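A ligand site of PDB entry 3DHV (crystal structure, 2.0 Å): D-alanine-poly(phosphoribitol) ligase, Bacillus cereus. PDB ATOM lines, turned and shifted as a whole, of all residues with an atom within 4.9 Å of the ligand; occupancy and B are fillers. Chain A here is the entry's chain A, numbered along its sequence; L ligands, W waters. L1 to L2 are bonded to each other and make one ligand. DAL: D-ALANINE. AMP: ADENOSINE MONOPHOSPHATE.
OG1 of Thr 381 lies within hydrogen-bond range of N of Asp 383 (3.0 Å). NH2 of Arg 397 lies within hydrogen-bond range of O of Thr 381, 2.8 Å away. The side-chain hydroxyl of Thr 293 sits close to the side-chain sulfur of Cys 269. N of Val 301 sits at hydrogen-bond distance from OD1 of Asp 197 (3.0 Å). OD2 of Asp 383 lies within salt-bridge range of NH2 of Arg 397 (2.8 Å). The side-chain carboxylate of Asp 383 sits at hydrogen-bond distance from the side-chain hydroxyl of Tyr 294 (2.6 Å).
The backbone carbonyl oxygen (O) of Glu 271 sits close to a nitrogen (N1) of AMP L2. Residues that only touch the ligand: Arg 397, Val 272, Cys 269, Tyr 294, Phe 196, Val 321 and Pro 296. Hydrophobic or aromatic side chains that line the ligand: Phe 196, Val 272, Tyr 294, Val 321 and Tyr 394. The nearest printed residue that does not touch the ligand is Leu 198 (4.01 Å).
The backbone carbonyl oxygen (O) of Thr 293 sits at hydrogen-bond distance from a nitrogen (N6) of AMP L2, 2.4 Å away. O3P of AMP L2 sits at hydrogen-bond distance from OG1 of Thr 297, 2.9 Å away. N of Thr 297 sits at hydrogen-bond distance from O3P of AMP L2 (3.2 Å). O2' of AMP L2 is in hydrogen-bond range of OH of Tyr 394, at 2.8 Å. N of Gly 270 sits at hydrogen-bond distance from N7 of AMP L2 (3.2 Å). N of DAL L1 sits at hydrogen-bond distance from O of Val 301. OD2 of Asp 197 is in salt-bridge range of N of DAL L1 (2.8 Å). A nitrogen (N6) of AMP L2 is in hydrogen-bond range of the side-chain amide oxygen (OD1) of Asn 292 (3.4 Å). OD1 of Asp 383 sits at hydrogen-bond distance from O3' of AMP L2 (2.6 Å). O1P of AMP L2 is in salt-bridge range of NZ of Lys 492, 3.2 Å away. The backbone carbonyl oxygen of Gly 295 lies close to a nitrogen (N) of DAL L1, at 3.1 Å.
Water W2 lies within hydrogen-bond range of the backbone NH of Leu 273 (2.9 Å), a nitrogen (N1) of AMP L2 (3.0 Å) and the side-chain amide nitrogen of Asn 292 (3.0 Å). Water W4 lies within hydrogen-bond range of N3 of AMP L2 (3.0 Å) and OH of Tyr 394 (3.3 Å). Water W3 lies within hydrogen-bond range of O of Glu 271, OD1 of Asn 292, N of Cys 269 and N6 of AMP L2.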
ATOM      1  N   THR A 152       6.978   2.721 -29.573  1.00  0.00           N
ATOM      2  CA  THR A 152       8.029   1.727 -29.342  1.00  0.00           C
ATOM      3  C   THR A 152       7.467   0.324 -29.601  1.00  0.00           C
ATOM      4  O   THR A 152       6.261   0.156 -29.765  1.00  0.00           O
ATOM      5  CB  THR A 152       8.572   1.782 -27.899  1.00  0.00           C
ATOM      6  OG1 THR A 152       7.485   1.658 -26.962  1.00  0.00           O
ATOM      7  CG2 THR A 152       9.303   3.091 -27.650  1.00  0.00           C
ATOM      8  N   PHE A 196      12.777   7.886 -33.388  1.00  0.00           N
ATOM      9  CA  PHE A 196      13.607   7.305 -32.312  1.00  0.00           C
ATOM     10  C   PHE A 196      13.920   8.465 -31.350  1.00  0.00           C
ATOM     11  O   PHE A 196      14.501   9.472 -31.759  1.00  0.00           O
ATOM     12  CB  PHE A 196      14.876   6.712 -32.950  1.00  0.00           C
ATOM     13  CG  PHE A 196      15.852   6.141 -31.962  1.00  0.00           C
ATOM     14  CD1 PHE A 196      15.438   5.559 -30.764  1.00  0.00           C
ATOM     15  CD2 PHE A 196      17.212   6.106 -32.280  1.00  0.00           C
ATOM     16  CE1 PHE A 196      16.347   4.961 -29.911  1.00  0.00           C
ATOM     17  CE2 PHE A 196      18.143   5.507 -31.421  1.00  0.00           C
ATOM     18  CZ  PHE A 196      17.707   4.931 -30.242  1.00  0.00           C
ATOM     19  N   ASP A 197      13.548   8.328 -30.075  1.00  0.00           N
ATOM     20  CA  ASP A 197      13.757   9.437 -29.134  1.00  0.00           C
ATOM     21  C   ASP A 197      15.191   9.863 -28.855  1.00  0.00           C
ATOM     22  O   ASP A 197      15.409  10.835 -28.141  1.00  0.00           O
ATOM     23  CB  ASP A 197      12.981   9.218 -27.820  1.00  0.00           C
ATOM     24  CG  ASP A 197      13.717   8.349 -26.817  1.00  0.00           C
ATOM     25  OD1 ASP A 197      13.316   8.382 -25.627  1.00  0.00           O
ATOM     26  OD2 ASP A 197      14.669   7.644 -27.183  1.00  0.00           O
ATOM     27  N   LEU A 198      16.165   9.160 -29.419  1.00  0.00           N
ATOM     28  CA  LEU A 198      17.546   9.583 -29.222  1.00  0.00           C
ATOM     29  C   LEU A 198      17.709  10.960 -29.873  1.00  0.00           C
ATOM     30  O   LEU A 198      18.487  11.806 -29.417  1.00  0.00           O
ATOM     31  CB  LEU A 198      18.531   8.587 -29.860  1.00  0.00           C
ATOM     32  CG  LEU A 198      20.000   9.013 -29.796  1.00  0.00           C
ATOM     33  CD1 LEU A 198      20.395   9.332 -28.364  1.00  0.00           C
ATOM     34  CD2 LEU A 198      20.881   7.908 -30.363  1.00  0.00           C
ATOM     35  N   CYS A 269      23.711   6.902 -26.101  1.00  0.00           N
ATOM     36  CA  CYS A 269      22.541   6.324 -25.445  1.00  0.00           C
ATOM     37  C   CYS A 269      21.940   5.264 -26.351  1.00  0.00           C
ATOM     38  O   CYS A 269      22.272   5.202 -27.532  1.00  0.00           O
ATOM     39  CB  CYS A 269      21.494   7.410 -25.163  1.00  0.00           C
ATOM     40  SG  CYS A 269      20.164   6.926 -24.022  1.00  0.00           S
ATOM     41  N   GLY A 270      21.069   4.413 -25.803  1.00  0.00           N
ATOM     42  CA  GLY A 270      20.425   3.399 -26.613  1.00  0.00           C
ATOM     43  C   GLY A 270      20.947   1.980 -26.528  1.00  0.00           C
ATOM     44  O   GLY A 270      20.154   1.044 -26.586  1.00  0.00           O
ATOM     45  N   GLU A 271      22.267   1.824 -26.426  1.00  0.00           N
ATOM     46  CA  GLU A 271      22.890   0.499 -26.319  1.00  0.00           C
ATOM     47  C   GLU A 271      24.110   0.554 -25.388  1.00  0.00           C
ATOM     48  O   GLU A 271      24.479   1.601 -24.874  1.00  0.00           O
ATOM     49  CB  GLU A 271      23.403   0.000 -27.678  1.00  0.00           C
ATOM     50  CG  GLU A 271      22.660   0.483 -28.903  1.00  0.00           C
ATOM     51  CD  GLU A 271      23.331  -0.006 -30.178  1.00  0.00           C
ATOM     52  OE1 GLU A 271      23.043  -1.144 -30.610  1.00  0.00           O
ATOM     53  OE2 GLU A 271      24.159   0.741 -30.740  1.00  0.00           O
ATOM     54  N   VAL A 272      24.752  -0.602 -25.217  1.00  0.00           N
ATOM     55  CA  VAL A 272      25.943  -0.690 -24.391  1.00  0.00           C
ATOM     56  C   VAL A 272      27.079   0.050 -25.082  1.00  0.00           C
ATOM     57  O   VAL A 272      27.328  -0.143 -26.270  1.00  0.00           O
ATOM     58  CB  VAL A 272      26.374  -2.157 -24.167  1.00  0.00           C
ATOM     59  CG1 VAL A 272      27.783  -2.201 -23.536  1.00  0.00           C
ATOM     60  CG2 VAL A 272      25.386  -2.874 -23.265  1.00  0.00           C
ATOM     61  N   LEU A 273      27.752   0.923 -24.350  1.00  0.00           N
ATOM     62  CA  LEU A 273      28.886   1.661 -24.897  1.00  0.00           C
ATOM     63  C   LEU A 273      30.094   0.858 -24.444  1.00  0.00           C
ATOM     64  O   LEU A 273      30.394   0.804 -23.255  1.00  0.00           O
ATOM     65  CB  LEU A 273      28.960   3.087 -24.326  1.00  0.00           C
ATOM     66  CG  LEU A 273      30.218   3.860 -24.723  1.00  0.00           C
ATOM     67  CD1 LEU A 273      30.227   4.090 -26.236  1.00  0.00           C
ATOM     68  CD2 LEU A 273      30.292   5.187 -23.948  1.00  0.00           C
ATOM     69  N   ASN A 292      28.243   8.830 -21.346  1.00  0.00           N
ATOM     70  CA  ASN A 292      27.426   7.644 -21.566  1.00  0.00           C
ATOM     71  C   ASN A 292      26.138   7.977 -20.814  1.00  0.00           C
ATOM     72  O   ASN A 292      26.196   8.573 -19.733  1.00  0.00           O
ATOM     73  CB  ASN A 292      28.062   6.369 -21.001  1.00  0.00           C
ATOM     74  CG  ASN A 292      27.308   5.100 -21.416  1.00  0.00           C
ATOM     75  OD1 ASN A 292      26.642   5.085 -22.450  1.00  0.00           O
ATOM     76  ND2 ASN A 292      27.440   4.029 -20.620  1.00  0.00           N
ATOM     77  N   THR A 293      24.992   7.644 -21.401  1.00  0.00           N
ATOM     78  CA  THR A 293      23.703   7.909 -20.780  1.00  0.00           C
ATOM     79  C   THR A 293      22.805   6.707 -20.941  1.00  0.00           C
ATOM     80  O   THR A 293      23.039   5.875 -21.811  1.00  0.00           O
ATOM     81  CB  THR A 293      23.040   9.147 -21.418  1.00  0.00           C
ATOM     82  OG1 THR A 293      22.715   8.860 -22.782  1.00  0.00           O
ATOM     83  CG2 THR A 293      23.993  10.333 -21.373  1.00  0.00           C
ATOM     84  N   TYR A 294      21.761   6.620 -20.121  1.00  0.00           N
ATOM     85  CA  TYR A 294      20.854   5.482 -20.173  1.00  0.00           C
ATOM     86  C   TYR A 294      19.413   5.839 -19.895  1.00  0.00           C
ATOM     87  O   TYR A 294      19.122   6.657 -19.026  1.00  0.00           O
ATOM     88  CB  TYR A 294      21.285   4.409 -19.161  1.00  0.00           C
ATOM     89  CG  TYR A 294      20.147   3.471 -18.737  1.00  0.00           C
ATOM     90  CD1 TYR A 294      19.942   2.250 -19.387  1.00  0.00           C
ATOM     91  CD2 TYR A 294      19.268   3.847 -17.727  1.00  0.00           C
ATOM     92  CE1 TYR A 294      18.871   1.421 -19.039  1.00  0.00           C
ATOM     93  CE2 TYR A 294      18.183   3.026 -17.375  1.00  0.00           C
ATOM     94  CZ  TYR A 294      17.998   1.818 -18.029  1.00  0.00           C
ATOM     95  OH  TYR A 294      16.931   1.020 -17.707  1.00  0.00           O
ATOM     96  N   GLY A 295      18.498   5.194 -20.615  1.00  0.00           N
ATOM     97  CA  GLY A 295      17.084   5.424 -20.394  1.00  0.00           C
ATOM     98  C   GLY A 295      16.157   4.871 -21.465  1.00  0.00           C
ATOM     99  O   GLY A 295      16.569   4.705 -22.616  1.00  0.00           O
ATOM    100  N   PRO A 296      14.901   4.560 -21.097  1.00  0.00           N
ATOM    101  CA  PRO A 296      13.900   4.033 -22.025  1.00  0.00           C
ATOM    102  C   PRO A 296      13.137   5.212 -22.581  1.00  0.00           C
ATOM    103  O   PRO A 296      13.158   6.296 -21.994  1.00  0.00           O
ATOM    104  CB  PRO A 296      13.021   3.168 -21.110  1.00  0.00           C
ATOM    105  CG  PRO A 296      12.984   3.989 -19.877  1.00  0.00           C
ATOM    106  CD  PRO A 296      14.458   4.393 -19.700  1.00  0.00           C
ATOM    107  N   THR A 297      12.459   5.016 -23.706  1.00  0.00           N
ATOM    108  CA  THR A 297      11.667   6.088 -24.294  1.00  0.00           C
ATOM    109  C   THR A 297      10.624   6.505 -23.251  1.00  0.00           C
ATOM    110  O   THR A 297      10.282   7.681 -23.122  1.00  0.00           O
ATOM    111  CB  THR A 297      10.948   5.591 -25.591  1.00  0.00           C
ATOM    112  OG1 THR A 297      11.935   5.117 -26.523  1.00  0.00           O
ATOM    113  CG2 THR A 297      10.171   6.720 -26.242  1.00  0.00           C
ATOM    114  N   GLU A 298      10.161   5.509 -22.488  1.00  0.00           N
ATOM    115  CA  GLU A 298       9.155   5.699 -21.436  1.00  0.00           C
ATOM    116  C   GLU A 298       9.572   6.664 -20.312  1.00  0.00           C
ATOM    117  O   GLU A 298       8.733   7.089 -19.507  1.00  0.00           O
ATOM    118  CB  GLU A 298       8.762   4.345 -20.822  1.00  0.00           C
ATOM    119  CG  GLU A 298       7.863   3.482 -21.725  1.00  0.00           C
ATOM    120  CD  GLU A 298       8.646   2.646 -22.752  1.00  0.00           C
ATOM    121  OE1 GLU A 298       9.863   2.821 -22.882  1.00  0.00           O
ATOM    122  OE2 GLU A 298       8.001   1.812 -23.440  1.00  0.00           O
ATOM    123  N   VAL A 301      13.836   9.889 -23.083  1.00  0.00           N
ATOM    124  CA  VAL A 301      15.200   9.810 -23.591  1.00  0.00           C
ATOM    125  C   VAL A 301      16.235   9.156 -22.685  1.00  0.00           C
ATOM    126  O   VAL A 301      16.674   8.041 -22.956  1.00  0.00           O
ATOM    127  CB  VAL A 301      15.716  11.217 -24.019  1.00  0.00           C
ATOM    128  CG1 VAL A 301      16.965  11.086 -24.882  1.00  0.00           C
ATOM    129  CG2 VAL A 301      14.622  11.959 -24.797  1.00  0.00           C
ATOM    130  N   ALA A 302      16.621   9.839 -21.614  1.00  0.00           N
ATOM    131  CA  ALA A 302      17.607   9.294 -20.693  1.00  0.00           C
ATOM    132  C   ALA A 302      17.453   9.935 -19.316  1.00  0.00           C
ATOM    133  O   ALA A 302      16.992  11.072 -19.217  1.00  0.00           O
ATOM    134  CB  ALA A 302      19.025   9.538 -21.225  1.00  0.00           C
ATOM    135  N   VAL A 321      26.336   3.213 -16.496  1.00  0.00           N
ATOM    136  CA  VAL A 321      25.536   4.069 -17.363  1.00  0.00           C
ATOM    137  C   VAL A 321      25.282   5.441 -16.756  1.00  0.00           C
ATOM    138  O   VAL A 321      24.659   6.303 -17.388  1.00  0.00           O
ATOM    139  CB  VAL A 321      24.199   3.412 -17.781  1.00  0.00           C
ATOM    140  CG1 VAL A 321      24.485   2.165 -18.624  1.00  0.00           C
ATOM    141  CG2 VAL A 321      23.365   3.058 -16.569  1.00  0.00           C
ATOM    142  N   THR A 381      11.467  -0.915 -16.235  1.00  0.00           N
ATOM    143  CA  THR A 381      12.178  -0.962 -17.510  1.00  0.00           C
ATOM    144  C   THR A 381      12.312  -2.302 -18.219  1.00  0.00           C
ATOM    145  O   THR A 381      12.422  -2.347 -19.449  1.00  0.00           O
ATOM    146  CB  THR A 381      13.610  -0.385 -17.371  1.00  0.00           C
ATOM    147  OG1 THR A 381      14.409  -1.241 -16.534  1.00  0.00           O
ATOM    148  CG2 THR A 381      13.560   1.017 -16.756  1.00  0.00           C
ATOM    149  N   ASP A 383      14.771  -3.976 -17.654  1.00  0.00           N
ATOM    150  CA  ASP A 383      16.235  -4.034 -17.675  1.00  0.00           C
ATOM    151  C   ASP A 383      16.759  -4.558 -16.346  1.00  0.00           C
ATOM    152  O   ASP A 383      16.168  -4.322 -15.294  1.00  0.00           O
ATOM    153  CB  ASP A 383      16.831  -2.645 -17.902  1.00  0.00           C
ATOM    154  CG  ASP A 383      16.604  -2.131 -19.299  1.00  0.00           C
ATOM    155  OD1 ASP A 383      16.483  -0.906 -19.460  1.00  0.00           O
ATOM    156  OD2 ASP A 383      16.564  -2.937 -20.249  1.00  0.00           O
ATOM    157  N   TYR A 394      24.299  -1.252 -15.884  1.00  0.00           N
ATOM    158  CA  TYR A 394      23.378  -1.986 -16.736  1.00  0.00           C
ATOM    159  C   TYR A 394      23.931  -3.380 -16.962  1.00  0.00           C
ATOM    160  O   TYR A 394      25.098  -3.522 -17.338  1.00  0.00           O
ATOM    161  CB  TYR A 394      23.266  -1.252 -18.072  1.00  0.00           C
ATOM    162  CG  TYR A 394      22.420  -1.937 -19.123  1.00  0.00           C
ATOM    163  CD1 TYR A 394      21.027  -1.806 -19.115  1.00  0.00           C
ATOM    164  CD2 TYR A 394      23.005  -2.690 -20.144  1.00  0.00           C
ATOM    165  CE1 TYR A 394      20.248  -2.394 -20.102  1.00  0.00           C
ATOM    166  CE2 TYR A 394      22.225  -3.273 -21.144  1.00  0.00           C
ATOM    167  CZ  TYR A 394      20.846  -3.118 -21.113  1.00  0.00           C
ATOM    168  OH  TYR A 394      20.072  -3.684 -22.100  1.00  0.00           O
ATOM    169  N   ARG A 397      18.975  -6.867 -20.799  1.00  0.00           N
ATOM    170  CA  ARG A 397      17.511  -6.961 -20.858  1.00  0.00           C
ATOM    171  C   ARG A 397      17.102  -8.253 -20.159  1.00  0.00           C
ATOM    172  O   ARG A 397      17.665  -9.307 -20.429  1.00  0.00           O
ATOM    173  CB  ARG A 397      17.032  -7.028 -22.317  1.00  0.00           C
ATOM    174  CG  ARG A 397      17.225  -5.744 -23.113  1.00  0.00           C
ATOM    175  CD  ARG A 397      16.279  -4.659 -22.617  1.00  0.00           C
ATOM    176  NE  ARG A 397      14.871  -5.015 -22.825  1.00  0.00           N
ATOM    177  CZ  ARG A 397      13.862  -4.400 -22.232  1.00  0.00           C
ATOM    178  NH1 ARG A 397      12.611  -4.777 -22.473  1.00  0.00           N
ATOM    179  NH2 ARG A 397      14.091  -3.420 -21.372  1.00  0.00           N
ATOM    180  N   LYS A 492      20.731   0.936 -34.100  1.00  0.00           N
ATOM    181  CA  LYS A 492      21.058  -0.096 -33.127  1.00  0.00           C
ATOM    182  C   LYS A 492      21.398  -1.424 -33.807  1.00  0.00           C
ATOM    183  O   LYS A 492      21.048  -1.644 -34.961  1.00  0.00           O
ATOM    184  CB  LYS A 492      19.881  -0.340 -32.169  1.00  0.00           C
ATOM    185  CG  LYS A 492      19.572   0.791 -31.195  1.00  0.00           C
ATOM    186  CD  LYS A 492      18.678   0.246 -30.082  1.00  0.00           C
ATOM    187  CE  LYS A 492      18.357   1.285 -29.013  1.00  0.00           C
ATOM    188  NZ  LYS A 492      17.187   2.100 -29.380  1.00  0.00           N
HETATM  189  N   DAL L   1      15.789   6.572 -24.902  1.00  0.00           N
HETATM  190  CA  DAL L   1      16.959   5.845 -25.404  1.00  0.00           C
HETATM  191  CB  DAL L   1      17.707   6.699 -26.421  1.00  0.00           C
HETATM  192  C   DAL L   1      16.489   4.554 -26.050  1.00  0.00           C
HETATM  193  O   DAL L   1      17.263   3.834 -26.683  1.00  0.00           O
HETATM  194  P   AMP L   2      14.549   2.775 -26.321  1.00  0.00           P
HETATM  195  O1P AMP L   2      14.442   2.581 -27.783  1.00  0.00           O
HETATM  196  O2P AMP L   2      15.107   4.257 -26.017  1.00  0.00           O
HETATM  197  O3P AMP L   2      13.171   2.629 -25.677  1.00  0.00           O
HETATM  198  O5' AMP L   2      15.573   1.653 -25.706  1.00  0.00           O
HETATM  199  C5' AMP L   2      15.930   1.639 -24.224  1.00  0.00           C
HETATM  200  C4' AMP L   2      16.614   0.526 -23.964  1.00  0.00           C
HETATM  201  O4' AMP L   2      17.977   0.647 -24.517  1.00  0.00           O
HETATM  202  C3' AMP L   2      16.787   0.356 -22.409  1.00  0.00           C
HETATM  203  O3' AMP L   2      15.696  -0.287 -21.852  1.00  0.00           O
HETATM  204  C2' AMP L   2      18.214  -0.308 -22.311  1.00  0.00           C
HETATM  205  O2' AMP L   2      18.026  -1.836 -22.466  1.00  0.00           O
HETATM  206  C1' AMP L   2      18.950   0.211 -23.546  1.00  0.00           C
HETATM  207  N9  AMP L   2      19.833   1.212 -23.226  1.00  0.00           N
HETATM  208  C8  AMP L   2      19.620   2.602 -23.244  1.00  0.00           C
HETATM  209  N7  AMP L   2      20.709   3.221 -22.877  1.00  0.00           N
HETATM  210  C5  AMP L   2      21.671   2.286 -22.619  1.00  0.00           C
HETATM  211  C6  AMP L   2      23.008   2.343 -22.203  1.00  0.00           C
HETATM  212  N6  AMP L   2      23.627   3.524 -21.972  1.00  0.00           N
HETATM  213  N1  AMP L   2      23.710   1.144 -22.022  1.00  0.00           N
HETATM  214  C2  AMP L   2      23.103  -0.110 -22.258  1.00  0.00           C
HETATM  215  N3  AMP L   2      21.804  -0.199 -22.666  1.00  0.00           N
HETATM  216  C4  AMP L   2      21.122   1.027 -22.831  1.00  0.00           C
HETATM  217  O   HOH W   1      15.323  -0.860 -28.052  1.00  0.00           O
HETATM  218  O   HOH W   2      26.644   1.350 -21.670  1.00  0.00           O
HETATM  219  O   HOH W   3      25.132   4.345 -24.739  1.00  0.00           O
HETATM  220  O   HOH W   4      21.517  -2.342 -24.695  1.00  0.00           O
